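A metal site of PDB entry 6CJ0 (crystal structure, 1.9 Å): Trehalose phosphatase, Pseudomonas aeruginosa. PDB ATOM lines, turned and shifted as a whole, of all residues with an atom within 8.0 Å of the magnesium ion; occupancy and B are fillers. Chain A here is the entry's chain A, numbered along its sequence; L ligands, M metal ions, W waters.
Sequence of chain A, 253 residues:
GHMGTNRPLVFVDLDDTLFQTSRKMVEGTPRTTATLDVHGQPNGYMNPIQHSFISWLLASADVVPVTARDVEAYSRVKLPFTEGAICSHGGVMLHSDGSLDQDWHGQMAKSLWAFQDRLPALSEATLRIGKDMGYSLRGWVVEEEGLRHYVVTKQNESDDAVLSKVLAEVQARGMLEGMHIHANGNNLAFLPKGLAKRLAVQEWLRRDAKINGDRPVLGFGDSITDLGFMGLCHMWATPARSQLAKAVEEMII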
ATOM      1  N   VAL A  12     -14.444 -12.619  -7.832  1.00  0.00           N
ATOM      2  CA  VAL A  12     -13.947 -11.452  -8.560  1.00  0.00           C
ATOM      3  C   VAL A  12     -14.678 -11.342  -9.883  1.00  0.00           C
ATOM      4  O   VAL A  12     -14.737 -12.306 -10.663  1.00  0.00           O
ATOM      5  CB  VAL A  12     -12.419 -11.505  -8.780  1.00  0.00           C
ATOM      6  CG1 VAL A  12     -11.670 -11.437  -7.456  1.00  0.00           C
ATOM      7  CG2 VAL A  12     -11.982 -12.760  -9.567  1.00  0.00           C
ATOM      8  N   ASP A  13     -15.259 -10.175 -10.136  1.00  0.00           N
ATOM      9  CA  ASP A  13     -15.616  -9.785 -11.490  1.00  0.00           C
ATOM     10  C   ASP A  13     -14.350  -9.709 -12.346  1.00  0.00           C
ATOM     11  O   ASP A  13     -13.231  -9.569 -11.832  1.00  0.00           O
ATOM     12  CB  ASP A  13     -16.360  -8.446 -11.439  1.00  0.00           C
ATOM     13  CG  ASP A  13     -16.771  -7.963 -12.789  1.00  0.00           C
ATOM     14  OD1 ASP A  13     -17.712  -8.535 -13.373  1.00  0.00           O
ATOM     15  OD2 ASP A  13     -16.174  -7.000 -13.274  1.00  0.00           O
ATOM     16  N   LEU A  14     -14.514  -9.820 -13.670  1.00  0.00           N
ATOM     17  CA  LEU A  14     -13.357  -9.805 -14.567  1.00  0.00           C
ATOM     18  C   LEU A  14     -13.202  -8.466 -15.302  1.00  0.00           C
ATOM     19  O   LEU A  14     -12.336  -7.658 -14.953  1.00  0.00           O
ATOM     20  CB  LEU A  14     -13.451 -10.954 -15.572  1.00  0.00           C
ATOM     21  CG  LEU A  14     -13.394 -12.369 -14.971  1.00  0.00           C
ATOM     22  CD1 LEU A  14     -13.358 -13.436 -16.088  1.00  0.00           C
ATOM     23  CD2 LEU A  14     -12.188 -12.517 -14.030  1.00  0.00           C
ATOM     24  N   ASP A  15     -14.028  -8.230 -16.326  1.00  0.00           N
ATOM     25  CA  ASP A  15     -13.828  -7.047 -17.153  1.00  0.00           C
ATOM     26  C   ASP A  15     -14.047  -5.778 -16.337  1.00  0.00           C
ATOM     27  O   ASP A  15     -15.030  -5.656 -15.608  1.00  0.00           O
ATOM     28  CB  ASP A  15     -14.773  -7.071 -18.357  1.00  0.00           C
ATOM     29  CG  ASP A  15     -14.511  -8.262 -19.267  1.00  0.00           C
ATOM     30  OD1 ASP A  15     -14.974  -9.394 -18.987  1.00  0.00           O
ATOM     31  OD2 ASP A  15     -13.815  -8.069 -20.287  1.00  0.00           O
ATOM     32  N   ASP A  16     -13.071  -4.859 -16.427  1.00  0.00           N
ATOM     33  CA  ASP A  16     -13.032  -3.552 -15.760  1.00  0.00           C
ATOM     34  C   ASP A  16     -12.817  -3.669 -14.254  1.00  0.00           C
ATOM     35  O   ASP A  16     -12.773  -2.635 -13.572  1.00  0.00           O
ATOM     36  CB  ASP A  16     -14.292  -2.737 -16.019  1.00  0.00           C
ATOM     37  CG  ASP A  16     -14.626  -2.672 -17.478  1.00  0.00           C
ATOM     38  OD1 ASP A  16     -13.819  -2.119 -18.248  1.00  0.00           O
ATOM     39  OD2 ASP A  16     -15.669  -3.232 -17.888  1.00  0.00           O
ATOM     40  N   THR A  17     -12.655  -4.863 -13.714  1.00  0.00           N
ATOM     41  CA  THR A  17     -12.172  -5.038 -12.347  1.00  0.00           C
ATOM     42  C   THR A  17     -10.725  -5.493 -12.322  1.00  0.00           C
ATOM     43  O   THR A  17      -9.907  -4.885 -11.624  1.00  0.00           O
ATOM     44  CB  THR A  17     -13.066  -6.027 -11.591  1.00  0.00           C
ATOM     45  OG1 THR A  17     -14.380  -5.476 -11.477  1.00  0.00           O
ATOM     46  CG2 THR A  17     -12.520  -6.308 -10.193  1.00  0.00           C
ATOM     47  N   LEU A  18     -10.375  -6.533 -13.085  1.00  0.00           N
ATOM     48  CA  LEU A  18      -9.008  -7.033 -13.118  1.00  0.00           C
ATOM     49  C   LEU A  18      -8.217  -6.550 -14.329  1.00  0.00           C
ATOM     50  O   LEU A  18      -6.975  -6.621 -14.305  1.00  0.00           O
ATOM     51  CB  LEU A  18      -8.989  -8.566 -13.128  1.00  0.00           C
ATOM     52  CG  LEU A  18      -9.660  -9.291 -11.956  1.00  0.00           C
ATOM     53  CD1 LEU A  18      -9.454 -10.825 -12.056  1.00  0.00           C
ATOM     54  CD2 LEU A  18      -9.141  -8.742 -10.627  1.00  0.00           C
ATOM     55  N   PHE A  19      -8.885  -6.085 -15.379  1.00  0.00           N
ATOM     56  CA  PHE A  19      -8.240  -5.724 -16.643  1.00  0.00           C
ATOM     57  C   PHE A  19      -9.244  -4.955 -17.490  1.00  0.00           C
ATOM     58  O   PHE A  19     -10.433  -4.899 -17.160  1.00  0.00           O
ATOM     59  CB  PHE A  19      -7.730  -6.964 -17.405  1.00  0.00           C
ATOM     60  CG  PHE A  19      -8.790  -8.010 -17.646  1.00  0.00           C
ATOM     61  CD1 PHE A  19      -9.777  -7.813 -18.614  1.00  0.00           C
ATOM     62  CD2 PHE A  19      -8.780  -9.202 -16.923  1.00  0.00           C
ATOM     63  CE1 PHE A  19     -10.758  -8.791 -18.835  1.00  0.00           C
ATOM     64  CE2 PHE A  19      -9.740 -10.186 -17.137  1.00  0.00           C
ATOM     65  CZ  PHE A  19     -10.733  -9.977 -18.094  1.00  0.00           C
ATOM     66  N   LYS A  24      -9.709   1.861 -22.967  1.00  0.00           N
ATOM     67  CA  LYS A  24      -9.965   2.328 -21.608  1.00  0.00           C
ATOM     68  C   LYS A  24      -8.686   2.607 -20.829  1.00  0.00           C
ATOM     69  O   LYS A  24      -8.753   2.812 -19.610  1.00  0.00           O
ATOM     70  CB  LYS A  24     -10.837   1.315 -20.861  1.00  0.00           C
ATOM     71  CG  LYS A  24     -12.263   1.275 -21.398  1.00  0.00           C
ATOM     72  CD  LYS A  24     -13.147   0.319 -20.618  1.00  0.00           C
ATOM     73  CE  LYS A  24     -14.577   0.319 -21.169  1.00  0.00           C
ATOM     74  NZ  LYS A  24     -15.476  -0.590 -20.381  1.00  0.00           N
ATOM     75  N   VAL A  66     -16.363 -14.404 -11.418  1.00  0.00           N
ATOM     76  CA  VAL A  66     -17.815 -14.315 -11.515  1.00  0.00           C
ATOM     77  C   VAL A  66     -18.105 -13.362 -12.670  1.00  0.00           C
ATOM     78  O   VAL A  66     -17.997 -12.145 -12.494  1.00  0.00           O
ATOM     79  CB  VAL A  66     -18.464 -13.827 -10.216  1.00  0.00           C
ATOM     80  CG1 VAL A  66     -19.981 -13.894 -10.316  1.00  0.00           C
ATOM     81  CG2 VAL A  66     -17.983 -14.654  -9.022  1.00  0.00           C
ATOM     82  N   THR A  67     -18.457 -13.897 -13.835  1.00  0.00           N
ATOM     83  CA  THR A  67     -18.356 -13.107 -15.062  1.00  0.00           C
ATOM     84  C   THR A  67     -19.585 -13.243 -15.958  1.00  0.00           C
ATOM     85  O   THR A  67     -20.269 -14.280 -15.980  1.00  0.00           O
ATOM     86  CB  THR A  67     -17.074 -13.471 -15.867  1.00  0.00           C
ATOM     87  OG1 THR A  67     -16.941 -12.589 -16.986  1.00  0.00           O
ATOM     88  CG2 THR A  67     -17.095 -14.908 -16.361  1.00  0.00           C
ATOM     89  N   ALA A  68     -19.850 -12.169 -16.699  1.00  0.00           N
ATOM     90  CA  ALA A  68     -20.830 -12.190 -17.771  1.00  0.00           C
ATOM     91  C   ALA A  68     -20.351 -12.984 -18.971  1.00  0.00           C
ATOM     92  O   ALA A  68     -21.186 -13.432 -19.777  1.00  0.00           O
ATOM     93  CB  ALA A  68     -21.167 -10.759 -18.217  1.00  0.00           C
ATOM     94  N   HIS A 182     -28.753  -5.131 -16.981  1.00  0.00           N
ATOM     95  CA  HIS A 182     -27.400  -4.676 -16.660  1.00  0.00           C
ATOM     96  C   HIS A 182     -26.974  -3.665 -17.709  1.00  0.00           C
ATOM     97  O   HIS A 182     -27.024  -3.959 -18.913  1.00  0.00           O
ATOM     98  CB  HIS A 182     -26.412  -5.844 -16.605  1.00  0.00           C
ATOM     99  CG  HIS A 182     -24.986  -5.416 -16.654  1.00  0.00           C
ATOM    100  ND1 HIS A 182     -24.334  -4.884 -15.553  1.00  0.00           N
ATOM    101  CD2 HIS A 182     -24.075  -5.418 -17.659  1.00  0.00           C
ATOM    102  CE1 HIS A 182     -23.090  -4.593 -15.886  1.00  0.00           C
ATOM    103  NE2 HIS A 182     -22.908  -4.908 -17.155  1.00  0.00           N
ATOM    104  N   ASN A 184     -23.607  -1.086 -18.313  1.00  0.00           N
ATOM    105  CA  ASN A 184     -22.333  -0.465 -17.945  1.00  0.00           C
ATOM    106  C   ASN A 184     -21.505  -0.324 -19.204  1.00  0.00           C
ATOM    107  O   ASN A 184     -21.273  -1.316 -19.902  1.00  0.00           O
ATOM    108  CB  ASN A 184     -21.584  -1.285 -16.883  1.00  0.00           C
ATOM    109  CG  ASN A 184     -20.395  -0.530 -16.311  1.00  0.00           C
ATOM    110  OD1 ASN A 184     -20.165   0.622 -16.662  1.00  0.00           O
ATOM    111  ND2 ASN A 184     -19.647  -1.165 -15.399  1.00  0.00           N
ATOM    112  N   LYS A 197     -25.664 -13.381 -11.235  1.00  0.00           N
ATOM    113  CA  LYS A 197     -24.430 -13.733 -10.519  1.00  0.00           C
ATOM    114  C   LYS A 197     -24.739 -14.063  -9.071  1.00  0.00           C
ATOM    115  O   LYS A 197     -24.125 -14.959  -8.480  1.00  0.00           O
ATOM    116  CB  LYS A 197     -23.417 -12.582 -10.606  1.00  0.00           C
ATOM    117  CG  LYS A 197     -22.917 -12.236 -12.014  1.00  0.00           C
ATOM    118  CD  LYS A 197     -21.891 -11.065 -11.943  1.00  0.00           C
ATOM    119  CE  LYS A 197     -21.168 -10.796 -13.266  1.00  0.00           C
ATOM    120  NZ  LYS A 197     -19.973  -9.892 -13.043  1.00  0.00           N
ATOM    121  N   PHE A 220     -15.280  -8.684  -5.189  1.00  0.00           N
ATOM    122  CA  PHE A 220     -14.670  -7.572  -5.918  1.00  0.00           C
ATOM    123  C   PHE A 220     -15.447  -7.352  -7.207  1.00  0.00           C
ATOM    124  O   PHE A 220     -15.566  -8.283  -8.014  1.00  0.00           O
ATOM    125  CB  PHE A 220     -13.223  -7.882  -6.301  1.00  0.00           C
ATOM    126  CG  PHE A 220     -12.240  -7.681  -5.210  1.00  0.00           C
ATOM    127  CD1 PHE A 220     -12.005  -8.685  -4.272  1.00  0.00           C
ATOM    128  CD2 PHE A 220     -11.488  -6.524  -5.148  1.00  0.00           C
ATOM    129  CE1 PHE A 220     -11.065  -8.508  -3.273  1.00  0.00           C
ATOM    130  CE2 PHE A 220     -10.554  -6.336  -4.138  1.00  0.00           C
ATOM    131  CZ  PHE A 220     -10.338  -7.329  -3.193  1.00  0.00           C
ATOM    132  N   GLY A 221     -15.946  -6.143  -7.425  1.00  0.00           N
ATOM    133  CA  GLY A 221     -16.674  -5.864  -8.642  1.00  0.00           C
ATOM    134  C   GLY A 221     -16.666  -4.389  -8.962  1.00  0.00           C
ATOM    135  O   GLY A 221     -16.398  -3.553  -8.107  1.00  0.00           O
ATOM    136  N   ASP A 222     -16.972  -4.074 -10.227  1.00  0.00           N
ATOM    137  CA  ASP A 222     -16.941  -2.679 -10.672  1.00  0.00           C
ATOM    138  C   ASP A 222     -18.302  -2.120 -11.047  1.00  0.00           C
ATOM    139  O   ASP A 222     -18.456  -0.895 -11.069  1.00  0.00           O
ATOM    140  CB  ASP A 222     -16.012  -2.517 -11.882  1.00  0.00           C
ATOM    141  CG  ASP A 222     -16.603  -3.133 -13.126  1.00  0.00           C
ATOM    142  OD1 ASP A 222     -16.670  -4.365 -13.166  1.00  0.00           O
ATOM    143  OD2 ASP A 222     -17.060  -2.404 -14.046  1.00  0.00           O
ATOM    144  N   SER A 223     -19.268  -2.966 -11.392  1.00  0.00           N
ATOM    145  CA  SER A 223     -20.576  -2.501 -11.838  1.00  0.00           C
ATOM    146  C   SER A 223     -21.557  -2.420 -10.671  1.00  0.00           C
ATOM    147  O   SER A 223     -21.466  -3.178  -9.691  1.00  0.00           O
ATOM    148  CB  SER A 223     -21.159  -3.431 -12.909  1.00  0.00           C
ATOM    149  OG  SER A 223     -20.381  -3.399 -14.108  1.00  0.00           O
ATOM    150  N   THR A 225     -24.537  -3.440 -10.764  1.00  0.00           N
ATOM    151  CA  THR A 225     -25.232  -4.719 -10.691  1.00  0.00           C
ATOM    152  C   THR A 225     -24.375  -5.808 -10.074  1.00  0.00           C
ATOM    153  O   THR A 225     -24.906  -6.859  -9.709  1.00  0.00           O
ATOM    154  CB  THR A 225     -25.680  -5.165 -12.073  1.00  0.00           C
ATOM    155  OG1 THR A 225     -24.535  -5.309 -12.919  1.00  0.00           O
ATOM    156  CG2 THR A 225     -26.665  -4.149 -12.686  1.00  0.00           C
ATOM    157  N   ASP A 226     -23.058  -5.596  -9.949  1.00  0.00           N
ATOM    158  CA  ASP A 226     -22.241  -6.526  -9.181  1.00  0.00           C
ATOM    159  C   ASP A 226     -22.559  -6.479  -7.686  1.00  0.00           C
ATOM    160  O   ASP A 226     -22.134  -7.364  -6.948  1.00  0.00           O
ATOM    161  CB  ASP A 226     -20.750  -6.244  -9.389  1.00  0.00           C
ATOM    162  CG  ASP A 226     -20.280  -6.622 -10.790  1.00  0.00           C
ATOM    163  OD1 ASP A 226     -20.855  -7.563 -11.389  1.00  0.00           O
ATOM    164  OD2 ASP A 226     -19.317  -5.998 -11.293  1.00  0.00           O
ATOM    165  N   PHE A 229     -24.095  -9.946  -6.107  1.00  0.00           N
ATOM    166  CA  PHE A 229     -23.305 -11.007  -5.500  1.00  0.00           C
ATOM    167  C   PHE A 229     -22.384 -10.456  -4.415  1.00  0.00           C
ATOM    168  O   PHE A 229     -22.088 -11.159  -3.433  1.00  0.00           O
ATOM    169  CB  PHE A 229     -22.525 -11.807  -6.574  1.00  0.00           C
ATOM    170  CG  PHE A 229     -21.221 -11.177  -7.044  1.00  0.00           C
ATOM    171  CD1 PHE A 229     -20.041 -11.361  -6.337  1.00  0.00           C
ATOM    172  CD2 PHE A 229     -21.168 -10.468  -8.235  1.00  0.00           C
ATOM    173  CE1 PHE A 229     -18.848 -10.824  -6.768  1.00  0.00           C
ATOM    174  CE2 PHE A 229     -19.968  -9.926  -8.684  1.00  0.00           C
ATOM    175  CZ  PHE A 229     -18.805 -10.106  -7.939  1.00  0.00           C
HETATM  176  C1  LIG L   1     -17.781  -9.002 -16.183  1.00  0.00           C
HETATM  177  O1  LIG L   1     -17.540  -7.715 -16.267  1.00  0.00           O
HETATM  178  O2  LIG L   1     -18.953  -9.465 -15.879  1.00  0.00           O
HETATM  179  O3  LIG L   1     -16.844  -9.873 -16.357  1.00  0.00           O
HETATM  180 MG    MG M   1     -17.087  -6.013 -14.830  1.00  0.00          MG
HETATM  181  O   HOH W   1     -17.682  -4.238 -16.163  1.00  0.00           O
HETATM  182  O   HOH W   2     -19.023  -5.973 -13.968  1.00  0.00           O
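The side-chain carboxylate (OD2) of Asp 13 sits close to the side-chain hydroxyl (OG1) of Thr 17, at 3.0 Å.
The side-chain carboxylate (OD1) of Asp 13 lies within salt-bridge range of the side-chain amino group (NZ) of Lys 197.
The backbone carbonyl oxygen (O) of Phe 220 sits at hydrogen-bond distance from the backbone NH (N) of Asp 13, at 2.9 Å.
The side-chain carboxylate (OD2) of Asp 226 is in hydrogen-bond range of the backbone NH (N) of Asp 222 (3.2 Å).
OD2 of Asp 222 lies within hydrogen-bond range of OG of Ser 223 (3.5 Å).
The backbone NH (N) of Asp 222 lies within hydrogen-bond range of the side-chain hydroxyl (OG1) of Thr 17 (3.2 Å).
The side-chain carboxylate (OD2) of Asp 222 is in hydrogen-bond range of the side-chain amide nitrogen (ND2) of Asn 184 (3.2 Å).
Within 4 Å of the magnesium ion: Asp 13, Asp 15 and Asp 222.
The magnesium ion is bound by OD2 of Asp 13 (2.1 Å), water W2 (2.1 Å), O of Asp 15 (2.2 Å), O1 of the ligand (2.3 Å), water W1 (2.3 Å) and OD1 of Asp 222 (2.4 Å).
The magnesium ion has six donor atoms within binding distance.
Water W1 lies within hydrogen-bond range of OD2 of Asp 16 (2.8 Å), OD2 of Asp 222 (2.9 Å) and OG of Ser 223 (3.5 Å).
Water W2 lies within hydrogen-bond range of OD2 of Asp 226, OG of Ser 223 and OD1 of Asp 13.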
